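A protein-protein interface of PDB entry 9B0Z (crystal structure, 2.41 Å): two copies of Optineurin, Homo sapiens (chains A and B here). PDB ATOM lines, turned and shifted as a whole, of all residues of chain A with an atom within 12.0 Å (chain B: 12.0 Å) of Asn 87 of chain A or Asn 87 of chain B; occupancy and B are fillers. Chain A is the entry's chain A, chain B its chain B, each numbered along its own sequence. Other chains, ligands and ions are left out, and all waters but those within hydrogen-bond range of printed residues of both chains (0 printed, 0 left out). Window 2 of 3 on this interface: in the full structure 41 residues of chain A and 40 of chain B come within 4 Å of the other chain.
ND2 of Asn 87 of chain B lies close to ND2 of Asn 87 of chain A (3.2 Å).
Among the printed residues, pairs that only touch across the chains: Gln 79 of chain A with Leu 80 of chain B, Leu 80 of chain A with Gln 79 of chain B, Leu 80 of chain A with Leu 80 of chain B, Leu 83 of chain A with Leu 83 of chain B and Leu 83 of chain A with Leu 84 of chain B.
Asn 87 of chain A touches one residue of chain B. Of the printed residues of chain A, Asn 87 of chain B touches Asn 87 (2.2 Å). Leu 83 of chain A touches two residues of chain B. No residue of chain B comes within 4 Å of Lys 85 of chain A. No residue of chain B comes within 4 Å of Ala 89 of chain A. Leu 83 of chain B touches one residue of chain A. Of the printed residues of chain A, Leu 84 of chain B touches Leu 83 (3.7 Å). No residue of chain A comes within 4 Å of Lys 85 of chain B. No residue of chain A comes within 4 Å of Glu 86 of chain B. No residue of chain A comes within 4 Å of Ala 89 of chain B. Of the printed residues of chain B, Gln 79 of chain A touches Leu 80 (3.6 Å). Of the printed residues of chain A, Gln 79 of chain B touches Leu 80 (3.7 Å). Printed residues of chain B within 4 Å of Leu 80 of chain A: Gln 79 (3.7 Å) and Leu 80 (3.7 Å). Of the printed residues of chain A, Leu 80 of chain B touches Gln 79 and Leu 80. Leu 78 of chain A touches none of the printed residues of chain B. The nearest residue of chain B that does not touch Asn 87 of chain A is Leu 83 of chain B (4.1 Å). The nearest residue of chain A that does not touch Asn 87 of chain B is Leu 83 of chain A (4.2 Å).
Of the 13 printed residues of chain A, 4 touch a printed residue of chain B. Printed residues of chain A that touch a printed residue of chain B: Gln 79, Leu 80, Leu 83 and Asn 87. Along chain A the printed residues that touch a printed residue of chain B span positions 79 to 87. Hydrophobic or aromatic side chains of chain B that line the printed part of chain A: Leu 80, Leu 83 and Leu 84. Along chain B the printed residues that touch a printed residue of chain A span positions 79 to 87.
Gln 79 of chain A touches Leu 80 of chain B, and with the chains exchanged Leu 80 of chain A touches Gln 79 of chain B. Leu 80 of chain B touches its own counterpart, Leu 80 of chain A. Leu 83 of chain A touches its own counterpart, Leu 83 of chain B. Asn 87 of chain A touches its own counterpart, Asn 87 of chain B. Of the 6 pairs that touch across the chains among the printed residues, 5 have their exchanged pair printed and touching as well.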
ATOM      1  N   LEU A  78      17.943 -13.315 -18.231  1.00  0.00           N
ATOM      2  CA  LEU A  78      16.937 -12.384 -17.735  1.00  0.00           C
ATOM      3  C   LEU A  78      16.724 -11.231 -18.708  1.00  0.00           C
ATOM      4  O   LEU A  78      15.582 -10.908 -19.051  1.00  0.00           O
ATOM      5  CB  LEU A  78      17.334 -11.871 -16.353  1.00  0.00           C
ATOM      6  CG  LEU A  78      16.411 -10.845 -15.703  1.00  0.00           C
ATOM      7  CD1 LEU A  78      16.379 -11.132 -14.214  1.00  0.00           C
ATOM      8  CD2 LEU A  78      16.857  -9.406 -15.977  1.00  0.00           C
ATOM      9  N   GLN A  79      17.811 -10.583 -19.142  1.00  0.00           N
ATOM     10  CA  GLN A  79      17.698  -9.531 -20.153  1.00  0.00           C
ATOM     11  C   GLN A  79      16.944 -10.031 -21.374  1.00  0.00           C
ATOM     12  O   GLN A  79      16.140  -9.300 -21.962  1.00  0.00           O
ATOM     13  CB  GLN A  79      19.078  -9.032 -20.560  1.00  0.00           C
ATOM     14  CG  GLN A  79      19.917  -8.490 -19.422  1.00  0.00           C
ATOM     15  CD  GLN A  79      21.249  -7.962 -19.907  1.00  0.00           C
ATOM     16  OE1 GLN A  79      22.128  -7.615 -19.110  1.00  0.00           O
ATOM     17  NE2 GLN A  79      21.413  -7.906 -21.226  1.00  0.00           N
ATOM     18  N   LEU A  80      17.186 -11.279 -21.764  1.00  0.00           N
ATOM     19  CA  LEU A  80      16.465 -11.848 -22.894  1.00  0.00           C
ATOM     20  C   LEU A  80      14.986 -12.023 -22.564  1.00  0.00           C
ATOM     21  O   LEU A  80      14.119 -11.643 -23.357  1.00  0.00           O
ATOM     22  CB  LEU A  80      17.111 -13.169 -23.299  1.00  0.00           C
ATOM     23  CG  LEU A  80      16.769 -13.738 -24.670  1.00  0.00           C
ATOM     24  CD1 LEU A  80      17.337 -12.845 -25.748  1.00  0.00           C
ATOM     25  CD2 LEU A  80      17.357 -15.134 -24.776  1.00  0.00           C
ATOM     26  N   ALA A  81      14.677 -12.605 -21.401  1.00  0.00           N
ATOM     27  CA  ALA A  81      13.280 -12.791 -21.012  1.00  0.00           C
ATOM     28  C   ALA A  81      12.562 -11.452 -20.882  1.00  0.00           C
ATOM     29  O   ALA A  81      11.438 -11.284 -21.372  1.00  0.00           O
ATOM     30  CB  ALA A  81      13.199 -13.576 -19.707  1.00  0.00           C
ATOM     31  N   VAL A  82      13.192 -10.491 -20.200  1.00  0.00           N
ATOM     32  CA  VAL A  82      12.628  -9.148 -20.079  1.00  0.00           C
ATOM     33  C   VAL A  82      12.351  -8.565 -21.458  1.00  0.00           C
ATOM     34  O   VAL A  82      11.247  -8.087 -21.744  1.00  0.00           O
ATOM     35  CB  VAL A  82      13.576  -8.244 -19.270  1.00  0.00           C
ATOM     36  CG1 VAL A  82      13.267  -6.776 -19.531  1.00  0.00           C
ATOM     37  CG2 VAL A  82      13.502  -8.575 -17.780  1.00  0.00           C
ATOM     38  N   LEU A  83      13.355  -8.608 -22.336  1.00  0.00           N
ATOM     39  CA  LEU A  83      13.229  -8.022 -23.666  1.00  0.00           C
ATOM     40  C   LEU A  83      12.085  -8.664 -24.442  1.00  0.00           C
ATOM     41  O   LEU A  83      11.412  -7.996 -25.233  1.00  0.00           O
ATOM     42  CB  LEU A  83      14.554  -8.166 -24.412  1.00  0.00           C
ATOM     43  CG  LEU A  83      14.763  -7.499 -25.769  1.00  0.00           C
ATOM     44  CD1 LEU A  83      14.349  -8.445 -26.888  1.00  0.00           C
ATOM     45  CD2 LEU A  83      14.012  -6.171 -25.848  1.00  0.00           C
ATOM     46  N   LEU A  84      11.866  -9.965 -24.240  1.00  0.00           N
ATOM     47  CA  LEU A  84      10.791 -10.662 -24.936  1.00  0.00           C
ATOM     48  C   LEU A  84       9.421 -10.186 -24.465  1.00  0.00           C
ATOM     49  O   LEU A  84       8.502 -10.028 -25.276  1.00  0.00           O
ATOM     50  CB  LEU A  84      10.940 -12.166 -24.732  1.00  0.00           C
ATOM     51  CG  LEU A  84      12.064 -12.821 -25.537  1.00  0.00           C
ATOM     52  CD1 LEU A  84      11.840 -14.315 -25.672  1.00  0.00           C
ATOM     53  CD2 LEU A  84      12.143 -12.178 -26.913  1.00  0.00           C
ATOM     54  N   LYS A  85       9.255  -9.970 -23.157  1.00  0.00           N
ATOM     55  CA  LYS A  85       8.007  -9.392 -22.663  1.00  0.00           C
ATOM     56  C   LYS A  85       7.761  -8.022 -23.290  1.00  0.00           C
ATOM     57  O   LYS A  85       6.675  -7.754 -23.820  1.00  0.00           O
ATOM     58  CB  LYS A  85       8.033  -9.296 -21.137  1.00  0.00           C
ATOM     59  N   GLU A  86       8.774  -7.150 -23.258  1.00  0.00           N
ATOM     60  CA  GLU A  86       8.641  -5.807 -23.822  1.00  0.00           C
ATOM     61  C   GLU A  86       8.282  -5.867 -25.302  1.00  0.00           C
ATOM     62  O   GLU A  86       7.391  -5.147 -25.766  1.00  0.00           O
ATOM     63  CB  GLU A  86       9.936  -5.019 -23.611  1.00  0.00           C
ATOM     64  CG  GLU A  86      10.392  -4.957 -22.160  1.00  0.00           C
ATOM     65  CD  GLU A  86      11.634  -4.100 -21.965  1.00  0.00           C
ATOM     66  OE1 GLU A  86      11.976  -3.809 -20.797  1.00  0.00           O
ATOM     67  OE2 GLU A  86      12.268  -3.719 -22.975  1.00  0.00           O
ATOM     68  N   ASN A  87       8.988  -6.702 -26.066  1.00  0.00           N
ATOM     69  CA  ASN A  87       8.669  -6.872 -27.478  1.00  0.00           C
ATOM     70  C   ASN A  87       7.275  -7.441 -27.701  1.00  0.00           C
ATOM     71  O   ASN A  87       6.762  -7.345 -28.820  1.00  0.00           O
ATOM     72  CB  ASN A  87       9.718  -7.759 -28.158  1.00  0.00           C
ATOM     73  CG  ASN A  87      10.951  -6.975 -28.549  1.00  0.00           C
ATOM     74  OD1 ASN A  87      11.057  -5.782 -28.266  1.00  0.00           O
ATOM     75  ND2 ASN A  87      11.901  -7.644 -29.199  1.00  0.00           N
ATOM     76  N   ASP A  88       6.646  -8.038 -26.684  1.00  0.00           N
ATOM     77  CA  ASP A  88       5.250  -8.407 -26.832  1.00  0.00           C
ATOM     78  C   ASP A  88       4.313  -7.284 -26.409  1.00  0.00           C
ATOM     79  O   ASP A  88       3.097  -7.404 -26.606  1.00  0.00           O
ATOM     80  CB  ASP A  88       4.937  -9.665 -26.014  1.00  0.00           C
ATOM     81  N   ALA A  89       4.851  -6.191 -25.857  1.00  0.00           N
ATOM     82  CA  ALA A  89       4.074  -4.966 -25.693  1.00  0.00           C
ATOM     83  C   ALA A  89       3.888  -4.253 -27.026  1.00  0.00           C
ATOM     84  O   ALA A  89       2.875  -3.574 -27.232  1.00  0.00           O
ATOM     85  CB  ALA A  89       4.740  -4.038 -24.673  1.00  0.00           C
ATOM     86  N   PHE A  90       4.859  -4.392 -27.929  1.00  0.00           N
ATOM     87  CA  PHE A  90       4.826  -3.775 -29.251  1.00  0.00           C
ATOM     88  C   PHE A  90       4.728  -2.253 -29.142  1.00  0.00           C
ATOM     89  O   PHE A  90       5.740  -1.569 -28.982  1.00  0.00           O
ATOM     90  CB  PHE A  90       3.661  -4.331 -30.080  1.00  0.00           C
ATOM     91  N   LEU B  78      24.209 -14.372 -28.288  1.00  0.00           N
ATOM     92  CA  LEU B  78      23.879 -14.285 -29.705  1.00  0.00           C
ATOM     93  C   LEU B  78      22.388 -14.051 -29.910  1.00  0.00           C
ATOM     94  O   LEU B  78      21.988 -13.172 -30.679  1.00  0.00           O
ATOM     95  CB  LEU B  78      24.309 -15.573 -30.399  1.00  0.00           C
ATOM     96  CG  LEU B  78      23.983 -15.684 -31.876  1.00  0.00           C
ATOM     97  CD1 LEU B  78      25.084 -14.977 -32.613  1.00  0.00           C
ATOM     98  CD2 LEU B  78      23.885 -17.143 -32.286  1.00  0.00           C
ATOM     99  N   GLN B  79      21.556 -14.857 -29.246  1.00  0.00           N
ATOM    100  CA  GLN B  79      20.106 -14.682 -29.284  1.00  0.00           C
ATOM    101  C   GLN B  79      19.700 -13.264 -28.900  1.00  0.00           C
ATOM    102  O   GLN B  79      18.731 -12.717 -29.437  1.00  0.00           O
ATOM    103  CB  GLN B  79      19.460 -15.710 -28.362  1.00  0.00           C
ATOM    104  CG  GLN B  79      19.856 -17.128 -28.751  1.00  0.00           C
ATOM    105  CD  GLN B  79      19.203 -18.191 -27.899  1.00  0.00           C
ATOM    106  OE1 GLN B  79      18.359 -17.901 -27.043  1.00  0.00           O
ATOM    107  NE2 GLN B  79      19.608 -19.439 -28.116  1.00  0.00           N
ATOM    108  N   LEU B  80      20.419 -12.665 -27.947  1.00  0.00           N
ATOM    109  CA  LEU B  80      20.156 -11.281 -27.558  1.00  0.00           C
ATOM    110  C   LEU B  80      20.484 -10.310 -28.686  1.00  0.00           C
ATOM    111  O   LEU B  80      19.695  -9.410 -28.994  1.00  0.00           O
ATOM    112  CB  LEU B  80      20.960 -10.926 -26.310  1.00  0.00           C
ATOM    113  CG  LEU B  80      20.575  -9.635 -25.586  1.00  0.00           C
ATOM    114  CD1 LEU B  80      19.219  -9.757 -24.898  1.00  0.00           C
ATOM    115  CD2 LEU B  80      21.672  -9.260 -24.583  1.00  0.00           C
ATOM    116  N   ALA B  81      21.656 -10.471 -29.308  1.00  0.00           N
ATOM    117  CA  ALA B  81      22.076  -9.563 -30.373  1.00  0.00           C
ATOM    118  C   ALA B  81      21.091  -9.577 -31.538  1.00  0.00           C
ATOM    119  O   ALA B  81      20.727  -8.518 -32.068  1.00  0.00           O
ATOM    120  CB  ALA B  81      23.480  -9.929 -30.846  1.00  0.00           C
ATOM    121  N   VAL B  82      20.669 -10.769 -31.966  1.00  0.00           N
ATOM    122  CA  VAL B  82      19.659 -10.869 -33.018  1.00  0.00           C
ATOM    123  C   VAL B  82      18.412 -10.082 -32.629  1.00  0.00           C
ATOM    124  O   VAL B  82      17.921  -9.242 -33.395  1.00  0.00           O
ATOM    125  CB  VAL B  82      19.325 -12.346 -33.300  1.00  0.00           C
ATOM    126  CG1 VAL B  82      17.979 -12.465 -34.007  1.00  0.00           C
ATOM    127  CG2 VAL B  82      20.435 -13.003 -34.115  1.00  0.00           C
ATOM    128  N   LEU B  83      17.882 -10.340 -31.430  1.00  0.00           N
ATOM    129  CA  LEU B  83      16.644  -9.683 -31.021  1.00  0.00           C
ATOM    130  C   LEU B  83      16.804  -8.171 -30.948  1.00  0.00           C
ATOM    131  O   LEU B  83      15.910  -7.428 -31.370  1.00  0.00           O
ATOM    132  CB  LEU B  83      16.163 -10.234 -29.681  1.00  0.00           C
ATOM    133  CG  LEU B  83      15.159 -11.379 -29.797  1.00  0.00           C
ATOM    134  CD1 LEU B  83      13.969 -10.924 -30.610  1.00  0.00           C
ATOM    135  CD2 LEU B  83      15.786 -12.626 -30.420  1.00  0.00           C
ATOM    136  N   LEU B  84      17.933  -7.686 -30.428  1.00  0.00           N
ATOM    137  CA  LEU B  84      18.096  -6.237 -30.344  1.00  0.00           C
ATOM    138  C   LEU B  84      18.306  -5.615 -31.718  1.00  0.00           C
ATOM    139  O   LEU B  84      17.754  -4.549 -32.006  1.00  0.00           O
ATOM    140  CB  LEU B  84      19.236  -5.868 -29.393  1.00  0.00           C
ATOM    141  CG  LEU B  84      18.886  -6.006 -27.904  1.00  0.00           C
ATOM    142  CD1 LEU B  84      19.779  -5.107 -27.041  1.00  0.00           C
ATOM    143  CD2 LEU B  84      17.393  -5.745 -27.623  1.00  0.00           C
ATOM    144  N   LYS B  85      19.094  -6.261 -32.581  1.00  0.00           N
ATOM    145  CA  LYS B  85      19.285  -5.740 -33.933  1.00  0.00           C
ATOM    146  C   LYS B  85      17.956  -5.607 -34.666  1.00  0.00           C
ATOM    147  O   LYS B  85      17.654  -4.552 -35.235  1.00  0.00           O
ATOM    148  CB  LYS B  85      20.241  -6.635 -34.716  1.00  0.00           C
ATOM    149  N   GLU B  86      17.147  -6.670 -34.659  1.00  0.00           N
ATOM    150  CA  GLU B  86      15.856  -6.637 -35.342  1.00  0.00           C
ATOM    151  C   GLU B  86      14.949  -5.555 -34.761  1.00  0.00           C
ATOM    152  O   GLU B  86      14.384  -4.737 -35.496  1.00  0.00           O
ATOM    153  CB  GLU B  86      15.185  -8.007 -35.255  1.00  0.00           C
ATOM    154  N   ASN B  87      14.796  -5.546 -33.438  1.00  0.00           N
ATOM    155  CA  ASN B  87      13.995  -4.530 -32.763  1.00  0.00           C
ATOM    156  C   ASN B  87      14.578  -3.127 -32.927  1.00  0.00           C
ATOM    157  O   ASN B  87      13.821  -2.152 -32.938  1.00  0.00           O
ATOM    158  CB  ASN B  87      13.906  -4.925 -31.278  1.00  0.00           C
ATOM    159  CG  ASN B  87      13.063  -3.978 -30.435  1.00  0.00           C
ATOM    160  OD1 ASN B  87      12.934  -2.790 -30.706  1.00  0.00           O
ATOM    161  ND2 ASN B  87      12.510  -4.523 -29.368  1.00  0.00           N
ATOM    162  N   ASP B  88      15.880  -3.009 -33.172  1.00  0.00           N
ATOM    163  CA  ASP B  88      16.534  -1.724 -33.390  1.00  0.00           C
ATOM    164  C   ASP B  88      16.522  -1.286 -34.845  1.00  0.00           C
ATOM    165  O   ASP B  88      17.249  -0.353 -35.201  1.00  0.00           O
ATOM    166  CB  ASP B  88      17.975  -1.751 -32.875  1.00  0.00           C
ATOM    167  N   ALA B  89      15.760  -1.958 -35.701  1.00  0.00           N
ATOM    168  CA  ALA B  89      15.559  -1.478 -37.065  1.00  0.00           C
ATOM    169  C   ALA B  89      14.783  -0.160 -37.064  1.00  0.00           C
ATOM    170  O   ALA B  89      13.561  -0.138 -37.200  1.00  0.00           O
ATOM    171  CB  ALA B  89      14.823  -2.526 -37.892  1.00  0.00           C
